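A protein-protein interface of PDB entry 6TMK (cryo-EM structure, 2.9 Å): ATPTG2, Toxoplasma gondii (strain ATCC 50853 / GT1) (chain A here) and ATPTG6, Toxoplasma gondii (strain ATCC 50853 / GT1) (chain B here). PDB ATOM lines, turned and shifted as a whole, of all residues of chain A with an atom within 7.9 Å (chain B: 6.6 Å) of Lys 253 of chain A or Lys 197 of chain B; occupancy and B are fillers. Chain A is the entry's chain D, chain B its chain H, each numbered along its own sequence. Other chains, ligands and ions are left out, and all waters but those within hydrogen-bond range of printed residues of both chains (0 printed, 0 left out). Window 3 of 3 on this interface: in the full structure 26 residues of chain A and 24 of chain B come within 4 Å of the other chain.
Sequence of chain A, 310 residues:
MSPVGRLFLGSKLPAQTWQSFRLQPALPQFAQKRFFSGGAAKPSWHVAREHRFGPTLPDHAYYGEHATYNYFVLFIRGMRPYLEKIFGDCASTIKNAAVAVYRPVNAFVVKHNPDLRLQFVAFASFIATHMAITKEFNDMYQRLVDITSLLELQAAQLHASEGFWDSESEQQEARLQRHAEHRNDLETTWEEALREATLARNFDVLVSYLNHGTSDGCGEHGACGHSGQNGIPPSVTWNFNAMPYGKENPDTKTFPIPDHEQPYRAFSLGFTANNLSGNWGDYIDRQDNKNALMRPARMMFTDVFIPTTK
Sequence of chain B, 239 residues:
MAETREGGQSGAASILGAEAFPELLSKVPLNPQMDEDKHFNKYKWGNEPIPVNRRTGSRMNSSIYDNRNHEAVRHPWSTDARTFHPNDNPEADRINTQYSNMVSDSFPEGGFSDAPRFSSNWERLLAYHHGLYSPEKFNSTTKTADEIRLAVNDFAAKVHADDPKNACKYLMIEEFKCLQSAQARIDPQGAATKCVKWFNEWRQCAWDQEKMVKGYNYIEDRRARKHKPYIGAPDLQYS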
ATOM      1  N   PRO A 244     -14.633   3.968  19.502  1.00  0.00           N
ATOM      2  CA  PRO A 244     -13.376   3.440  18.980  1.00  0.00           C
ATOM      3  C   PRO A 244     -12.178   3.844  19.821  1.00  0.00           C
ATOM      4  O   PRO A 244     -12.190   4.837  20.550  1.00  0.00           O
ATOM      5  CB  PRO A 244     -13.302   4.061  17.584  1.00  0.00           C
ATOM      6  CG  PRO A 244     -13.991   5.343  17.736  1.00  0.00           C
ATOM      7  CD  PRO A 244     -15.122   5.085  18.682  1.00  0.00           C
ATOM      8  N   GLY A 246      -7.652   3.616  19.440  1.00  0.00           N
ATOM      9  CA  GLY A 246      -6.451   3.206  18.753  1.00  0.00           C
ATOM     10  C   GLY A 246      -5.542   4.350  18.390  1.00  0.00           C
ATOM     11  O   GLY A 246      -5.999   5.404  17.945  1.00  0.00           O
ATOM     12  N   LYS A 247      -4.239   4.146  18.571  1.00  0.00           N
ATOM     13  CA  LYS A 247      -3.275   5.125  18.096  1.00  0.00           C
ATOM     14  C   LYS A 247      -3.296   5.222  16.577  1.00  0.00           C
ATOM     15  O   LYS A 247      -3.259   6.322  16.017  1.00  0.00           O
ATOM     16  CB  LYS A 247      -1.882   4.747  18.592  1.00  0.00           C
ATOM     17  CG  LYS A 247      -0.872   5.857  18.494  1.00  0.00           C
ATOM     18  CD  LYS A 247       0.537   5.318  18.395  1.00  0.00           C
ATOM     19  CE  LYS A 247       1.546   6.286  18.983  1.00  0.00           C
ATOM     20  NZ  LYS A 247       1.283   7.698  18.589  1.00  0.00           N
ATOM     21  N   GLU A 248      -3.359   4.079  15.899  1.00  0.00           N
ATOM     22  CA  GLU A 248      -3.369   4.023  14.447  1.00  0.00           C
ATOM     23  C   GLU A 248      -4.755   3.812  13.856  1.00  0.00           C
ATOM     24  O   GLU A 248      -4.894   3.815  12.631  1.00  0.00           O
ATOM     25  CB  GLU A 248      -2.440   2.906  13.969  1.00  0.00           C
ATOM     26  CG  GLU A 248      -1.104   2.882  14.682  1.00  0.00           C
ATOM     27  CD  GLU A 248      -1.093   1.919  15.849  1.00  0.00           C
ATOM     28  OE1 GLU A 248      -2.157   1.740  16.481  1.00  0.00           O
ATOM     29  OE2 GLU A 248      -0.023   1.347  16.141  1.00  0.00           O
ATOM     30  N   ASN A 249      -5.771   3.627  14.680  1.00  0.00           N
ATOM     31  CA  ASN A 249      -7.113   3.392  14.171  1.00  0.00           C
ATOM     32  C   ASN A 249      -7.666   4.653  13.526  1.00  0.00           C
ATOM     33  O   ASN A 249      -7.784   5.681  14.204  1.00  0.00           O
ATOM     34  CB  ASN A 249      -8.016   2.932  15.299  1.00  0.00           C
ATOM     35  CG  ASN A 249      -9.362   2.468  14.812  1.00  0.00           C
ATOM     36  OD1 ASN A 249      -9.580   2.284  13.616  1.00  0.00           O
ATOM     37  ND2 ASN A 249     -10.274   2.261  15.743  1.00  0.00           N
ATOM     38  N   PRO A 250      -8.018   4.631  12.239  1.00  0.00           N
ATOM     39  CA  PRO A 250      -8.560   5.834  11.603  1.00  0.00           C
ATOM     40  C   PRO A 250     -10.021   6.110  11.913  1.00  0.00           C
ATOM     41  O   PRO A 250     -10.569   7.084  11.385  1.00  0.00           O
ATOM     42  CB  PRO A 250      -8.361   5.535  10.116  1.00  0.00           C
ATOM     43  CG  PRO A 250      -8.484   4.074  10.036  1.00  0.00           C
ATOM     44  CD  PRO A 250      -7.807   3.556  11.258  1.00  0.00           C
ATOM     45  N   ASP A 251     -10.665   5.295  12.743  1.00  0.00           N
ATOM     46  CA  ASP A 251     -11.997   5.626  13.229  1.00  0.00           C
ATOM     47  C   ASP A 251     -11.962   6.714  14.286  1.00  0.00           C
ATOM     48  O   ASP A 251     -13.021   7.157  14.739  1.00  0.00           O
ATOM     49  CB  ASP A 251     -12.686   4.381  13.788  1.00  0.00           C
ATOM     50  CG  ASP A 251     -12.758   3.251  12.783  1.00  0.00           C
ATOM     51  OD1 ASP A 251     -12.342   3.449  11.621  1.00  0.00           O
ATOM     52  OD2 ASP A 251     -13.239   2.160  13.152  1.00  0.00           O
ATOM     53  N   THR A 252     -10.768   7.156  14.674  1.00  0.00           N
ATOM     54  CA  THR A 252     -10.582   8.239  15.624  1.00  0.00           C
ATOM     55  C   THR A 252      -9.979   9.491  15.012  1.00  0.00           C
ATOM     56  O   THR A 252      -9.905  10.515  15.695  1.00  0.00           O
ATOM     57  CB  THR A 252      -9.678   7.774  16.770  1.00  0.00           C
ATOM     58  OG1 THR A 252      -8.494   7.180  16.227  1.00  0.00           O
ATOM     59  CG2 THR A 252     -10.371   6.770  17.629  1.00  0.00           C
ATOM     60  N   LYS A 253      -9.549   9.444  13.757  1.00  0.00           N
ATOM     61  CA  LYS A 253      -8.806  10.536  13.142  1.00  0.00           C
ATOM     62  C   LYS A 253      -9.738  11.351  12.258  1.00  0.00           C
ATOM     63  O   LYS A 253     -10.246  10.851  11.251  1.00  0.00           O
ATOM     64  CB  LYS A 253      -7.641   9.994  12.319  1.00  0.00           C
ATOM     65  CG  LYS A 253      -6.741   9.037  13.048  1.00  0.00           C
ATOM     66  CD  LYS A 253      -5.653   8.539  12.130  1.00  0.00           C
ATOM     67  CE  LYS A 253      -4.789   7.494  12.793  1.00  0.00           C
ATOM     68  NZ  LYS A 253      -4.286   6.525  11.785  1.00  0.00           N
ATOM     69  N   THR A 254      -9.965  12.605  12.640  1.00  0.00           N
ATOM     70  CA  THR A 254     -10.681  13.558  11.803  1.00  0.00           C
ATOM     71  C   THR A 254      -9.715  14.484  11.076  1.00  0.00           C
ATOM     72  O   THR A 254      -9.678  14.524   9.843  1.00  0.00           O
ATOM     73  CB  THR A 254     -11.654  14.373  12.656  1.00  0.00           C
ATOM     74  OG1 THR A 254     -10.992  14.813  13.845  1.00  0.00           O
ATOM     75  CG2 THR A 254     -12.846  13.546  13.022  1.00  0.00           C
ATOM     76  N   PHE A 255      -8.913  15.214  11.836  1.00  0.00           N
ATOM     77  CA  PHE A 255      -7.889  16.111  11.341  1.00  0.00           C
ATOM     78  C   PHE A 255      -6.614  15.872  12.130  1.00  0.00           C
ATOM     79  O   PHE A 255      -6.672  15.506  13.308  1.00  0.00           O
ATOM     80  CB  PHE A 255      -8.325  17.574  11.486  1.00  0.00           C
ATOM     81  CG  PHE A 255      -9.620  17.888  10.805  1.00  0.00           C
ATOM     82  CD1 PHE A 255      -9.661  18.152   9.453  1.00  0.00           C
ATOM     83  CD2 PHE A 255     -10.801  17.898  11.515  1.00  0.00           C
ATOM     84  CE1 PHE A 255     -10.848  18.431   8.829  1.00  0.00           C
ATOM     85  CE2 PHE A 255     -11.989  18.175  10.893  1.00  0.00           C
ATOM     86  CZ  PHE A 255     -12.013  18.440   9.548  1.00  0.00           C
ATOM     87  N   PRO A 256      -5.452  16.063  11.515  1.00  0.00           N
ATOM     88  CA  PRO A 256      -4.204  15.819  12.240  1.00  0.00           C
ATOM     89  C   PRO A 256      -4.009  16.808  13.374  1.00  0.00           C
ATOM     90  O   PRO A 256      -4.298  18.000  13.247  1.00  0.00           O
ATOM     91  CB  PRO A 256      -3.135  15.978  11.156  1.00  0.00           C
ATOM     92  CG  PRO A 256      -3.756  16.880  10.162  1.00  0.00           C
ATOM     93  CD  PRO A 256      -5.201  16.519  10.141  1.00  0.00           C
ATOM     94  N   ILE A 257      -3.518  16.293  14.493  1.00  0.00           N
ATOM     95  CA  ILE A 257      -3.239  17.104  15.673  1.00  0.00           C
ATOM     96  C   ILE A 257      -1.821  17.642  15.544  1.00  0.00           C
ATOM     97  O   ILE A 257      -0.904  16.880  15.206  1.00  0.00           O
ATOM     98  CB  ILE A 257      -3.442  16.291  16.958  1.00  0.00           C
ATOM     99  CG1 ILE A 257      -4.931  16.013  17.140  1.00  0.00           C
ATOM    100  CG2 ILE A 257      -2.890  17.043  18.156  1.00  0.00           C
ATOM    101  CD1 ILE A 257      -5.222  14.833  17.993  1.00  0.00           C
ATOM    102  N   CYS B 178     -20.338   9.382   5.867  1.00  0.00           N
ATOM    103  CA  CYS B 178     -19.653   8.223   6.416  1.00  0.00           C
ATOM    104  C   CYS B 178     -20.646   7.134   6.792  1.00  0.00           C
ATOM    105  O   CYS B 178     -20.372   5.947   6.586  1.00  0.00           O
ATOM    106  CB  CYS B 178     -18.797   8.643   7.612  1.00  0.00           C
ATOM    107  SG  CYS B 178     -17.360   9.641   7.178  1.00  0.00           S
ATOM    108  N   ALA B 192     -21.927   3.579  13.239  1.00  0.00           N
ATOM    109  CA  ALA B 192     -21.870   4.603  14.269  1.00  0.00           C
ATOM    110  C   ALA B 192     -20.480   4.639  14.873  1.00  0.00           C
ATOM    111  O   ALA B 192     -19.950   5.712  15.196  1.00  0.00           O
ATOM    112  CB  ALA B 192     -22.927   4.324  15.331  1.00  0.00           C
ATOM    113  N   THR B 193     -19.858   3.463  14.989  1.00  0.00           N
ATOM    114  CA  THR B 193     -18.484   3.387  15.468  1.00  0.00           C
ATOM    115  C   THR B 193     -17.532   4.183  14.583  1.00  0.00           C
ATOM    116  O   THR B 193     -16.507   4.677  15.065  1.00  0.00           O
ATOM    117  CB  THR B 193     -18.040   1.928  15.535  1.00  0.00           C
ATOM    118  OG1 THR B 193     -18.790   1.237  16.536  1.00  0.00           O
ATOM    119  CG2 THR B 193     -16.581   1.830  15.867  1.00  0.00           C
ATOM    120  N   LYS B 194     -17.842   4.313  13.293  1.00  0.00           N
ATOM    121  CA  LYS B 194     -17.030   5.101  12.375  1.00  0.00           C
ATOM    122  C   LYS B 194     -17.387   6.580  12.366  1.00  0.00           C
ATOM    123  O   LYS B 194     -16.517   7.415  12.101  1.00  0.00           O
ATOM    124  CB  LYS B 194     -17.180   4.566  10.953  1.00  0.00           C
ATOM    125  CG  LYS B 194     -17.132   3.072  10.827  1.00  0.00           C
ATOM    126  CD  LYS B 194     -15.813   2.496  11.208  1.00  0.00           C
ATOM    127  CE  LYS B 194     -15.573   1.210  10.455  1.00  0.00           C
ATOM    128  NZ  LYS B 194     -16.755   0.315  10.505  1.00  0.00           N
ATOM    129  N   CYS B 195     -18.645   6.922  12.624  1.00  0.00           N
ATOM    130  CA  CYS B 195     -19.148   8.269  12.378  1.00  0.00           C
ATOM    131  C   CYS B 195     -19.259   9.120  13.640  1.00  0.00           C
ATOM    132  O   CYS B 195     -19.509  10.339  13.544  1.00  0.00           O
ATOM    133  CB  CYS B 195     -20.504   8.183  11.677  1.00  0.00           C
ATOM    134  SG  CYS B 195     -20.394   7.313  10.106  1.00  0.00           S
ATOM    135  N   VAL B 196     -19.081   8.527  14.821  1.00  0.00           N
ATOM    136  CA  VAL B 196     -19.263   9.332  16.011  1.00  0.00           C
ATOM    137  C   VAL B 196     -18.165  10.379  16.127  1.00  0.00           C
ATOM    138  O   VAL B 196     -18.340  11.368  16.843  1.00  0.00           O
ATOM    139  CB  VAL B 196     -19.350   8.423  17.252  1.00  0.00           C
ATOM    140  CG1 VAL B 196     -18.071   7.661  17.467  1.00  0.00           C
ATOM    141  CG2 VAL B 196     -19.700   9.234  18.472  1.00  0.00           C
ATOM    142  N   LYS B 197     -17.042  10.212  15.428  1.00  0.00           N
ATOM    143  CA  LYS B 197     -15.998  11.232  15.486  1.00  0.00           C
ATOM    144  C   LYS B 197     -16.485  12.527  14.850  1.00  0.00           C
ATOM    145  O   LYS B 197     -16.245  13.623  15.374  1.00  0.00           O
ATOM    146  CB  LYS B 197     -14.733  10.754  14.789  1.00  0.00           C
ATOM    147  CG  LYS B 197     -14.937  10.327  13.380  1.00  0.00           C
ATOM    148  CD  LYS B 197     -13.645   9.929  12.754  1.00  0.00           C
ATOM    149  CE  LYS B 197     -13.865   9.283  11.427  1.00  0.00           C
ATOM    150  NZ  LYS B 197     -12.596   8.956  10.769  1.00  0.00           N
ATOM    151  N   TRP B 198     -17.178  12.413  13.717  1.00  0.00           N
ATOM    152  CA  TRP B 198     -17.714  13.587  13.052  1.00  0.00           C
ATOM    153  C   TRP B 198     -18.878  14.157  13.829  1.00  0.00           C
ATOM    154  O   TRP B 198     -19.079  15.378  13.841  1.00  0.00           O
ATOM    155  CB  TRP B 198     -18.154  13.257  11.632  1.00  0.00           C
ATOM    156  CG  TRP B 198     -17.048  12.859  10.753  1.00  0.00           C
ATOM    157  CD1 TRP B 198     -16.868  11.654  10.162  1.00  0.00           C
ATOM    158  CD2 TRP B 198     -15.942  13.667  10.365  1.00  0.00           C
ATOM    159  NE1 TRP B 198     -15.717  11.656   9.427  1.00  0.00           N
ATOM    160  CE2 TRP B 198     -15.128  12.887   9.535  1.00  0.00           C
ATOM    161  CE3 TRP B 198     -15.559  14.979  10.642  1.00  0.00           C
ATOM    162  CZ2 TRP B 198     -13.959  13.372   8.976  1.00  0.00           C
ATOM    163  CZ3 TRP B 198     -14.400  15.455  10.085  1.00  0.00           C
ATOM    164  CH2 TRP B 198     -13.614  14.655   9.263  1.00  0.00           C
ATOM    165  N   PHE B 199     -19.627  13.301  14.518  1.00  0.00           N
ATOM    166  CA  PHE B 199     -20.646  13.831  15.414  1.00  0.00           C
ATOM    167  C   PHE B 199     -20.017  14.657  16.531  1.00  0.00           C
ATOM    168  O   PHE B 199     -20.527  15.724  16.890  1.00  0.00           O
ATOM    169  CB  PHE B 199     -21.476  12.701  16.003  1.00  0.00           C
ATOM    170  CG  PHE B 199     -22.436  13.153  17.047  1.00  0.00           C
ATOM    171  CD1 PHE B 199     -23.580  13.826  16.691  1.00  0.00           C
ATOM    172  CD2 PHE B 199     -22.189  12.931  18.381  1.00  0.00           C
ATOM    173  CE1 PHE B 199     -24.460  14.250  17.635  1.00  0.00           C
ATOM    174  CE2 PHE B 199     -23.069  13.357  19.329  1.00  0.00           C
ATOM    175  CZ  PHE B 199     -24.207  14.020  18.954  1.00  0.00           C
ATOM    176  N   ASN B 200     -18.913  14.175  17.096  1.00  0.00           N
ATOM    177  CA  ASN B 200     -18.212  14.918  18.134  1.00  0.00           C
ATOM    178  C   ASN B 200     -17.672  16.247  17.610  1.00  0.00           C
ATOM    179  O   ASN B 200     -17.743  17.274  18.300  1.00  0.00           O
ATOM    180  CB  ASN B 200     -17.091  14.044  18.691  1.00  0.00           C
ATOM    181  CG  ASN B 200     -16.405  14.651  19.880  1.00  0.00           C
ATOM    182  OD1 ASN B 200     -17.046  15.095  20.833  1.00  0.00           O
ATOM    183  ND2 ASN B 200     -15.085  14.669  19.838  1.00  0.00           N
ATOM    184  N   GLU B 201     -17.136  16.254  16.389  1.00  0.00           N
ATOM    185  CA  GLU B 201     -16.644  17.504  15.818  1.00  0.00           C
ATOM    186  C   GLU B 201     -17.780  18.497  15.593  1.00  0.00           C
ATOM    187  O   GLU B 201     -17.617  19.701  15.823  1.00  0.00           O
ATOM    188  CB  GLU B 201     -15.919  17.236  14.505  1.00  0.00           C
ATOM    189  CG  GLU B 201     -14.600  16.531  14.633  1.00  0.00           C
ATOM    190  CD  GLU B 201     -13.513  17.395  15.234  1.00  0.00           C
ATOM    191  OE1 GLU B 201     -13.342  18.545  14.778  1.00  0.00           O
ATOM    192  OE2 GLU B 201     -12.824  16.925  16.163  1.00  0.00           O
ATOM    193  N   TRP B 202     -18.939  18.012  15.144  1.00  0.00           N
ATOM    194  CA  TRP B 202     -20.108  18.873  15.012  1.00  0.00           C
ATOM    195  C   TRP B 202     -20.535  19.432  16.365  1.00  0.00           C
ATOM    196  O   TRP B 202     -20.900  20.608  16.479  1.00  0.00           O
ATOM    197  CB  TRP B 202     -21.246  18.098  14.348  1.00  0.00           C
ATOM    198  CG  TRP B 202     -22.567  18.770  14.412  1.00  0.00           C
ATOM    199  CD1 TRP B 202     -23.088  19.615  13.491  1.00  0.00           C
ATOM    200  CD2 TRP B 202     -23.548  18.650  15.444  1.00  0.00           C
ATOM    201  NE1 TRP B 202     -24.324  20.043  13.882  1.00  0.00           N
ATOM    202  CE2 TRP B 202     -24.631  19.465  15.082  1.00  0.00           C
ATOM    203  CE3 TRP B 202     -23.613  17.941  16.644  1.00  0.00           C
ATOM    204  CZ2 TRP B 202     -25.764  19.584  15.869  1.00  0.00           C
ATOM    205  CZ3 TRP B 202     -24.738  18.066  17.420  1.00  0.00           C
ATOM    206  CH2 TRP B 202     -25.797  18.878  17.030  1.00  0.00           C
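NZ of Lys 197 of chain B is in hydrogen-bond range of O of Pro 250 of chain A (2.8 Å).
The backbone carbonyl oxygen (O) of Lys 253 of chain A sits at hydrogen-bond distance from the side-chain amino group (NZ) of Lys 197 of chain B, at 3.1 Å.
SG of Cys 178 of chain B sits at hydrogen-bond distance from NE1 of Trp 198 of chain B.
NZ of Lys 253 of chain A sits at hydrogen-bond distance from O of Glu 248 of chain A (2.9 Å).
The side-chain amide oxygen (OD1) of Asn 249 of chain A lies close to the backbone NH (N) of Asp 251 of chain A (3.3 Å).
Among the printed residues, pairs that only touch across the chains: Asp 251 of chain A with Lys 194 of chain B, Asp 251 of chain A with Lys 197 of chain B, Thr 254 of chain A with Glu 201 of chain B, Thr 254 of chain A with Lys 197 of chain B, Phe 255 of chain A with Trp 198 of chain B, Pro 244 of chain A with Thr 193 of chain B and Thr 254 of chain A with Trp 198 of chain B.
Asn 249 of chain A touches none of the printed residues of chain B.
Printed residues of chain B within 4 Å of Pro 250 of chain A: Lys 197.
Of chain B, only Lys 197 comes within 4 Å of Lys 253 of chain A.
Printed residues of chain B within 4 Å of Phe 255 of chain A: Trp 198 (3.7 Å).
Lys 197 of chain B touches four residues of chain A.
The nearest residue of chain B that does not touch Lys 253 of chain A is Trp 198 of chain B (5.0 Å).
The nearest residue of chain A that does not touch Lys 197 of chain B is Thr 252 of chain A (4.3 Å).
Hydrophobic or aromatic side chains of chain A within 4 Å of the printed part of chain B: Pro 244 and Phe 255.
Hydrophobic or aromatic side chains of chain B that line the printed part of chain A: Trp 198.
Among the printed residues, no Asp or Glu carboxylate lies within 4 Å of a Lys or Arg side-chain nitrogen of the other chain.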
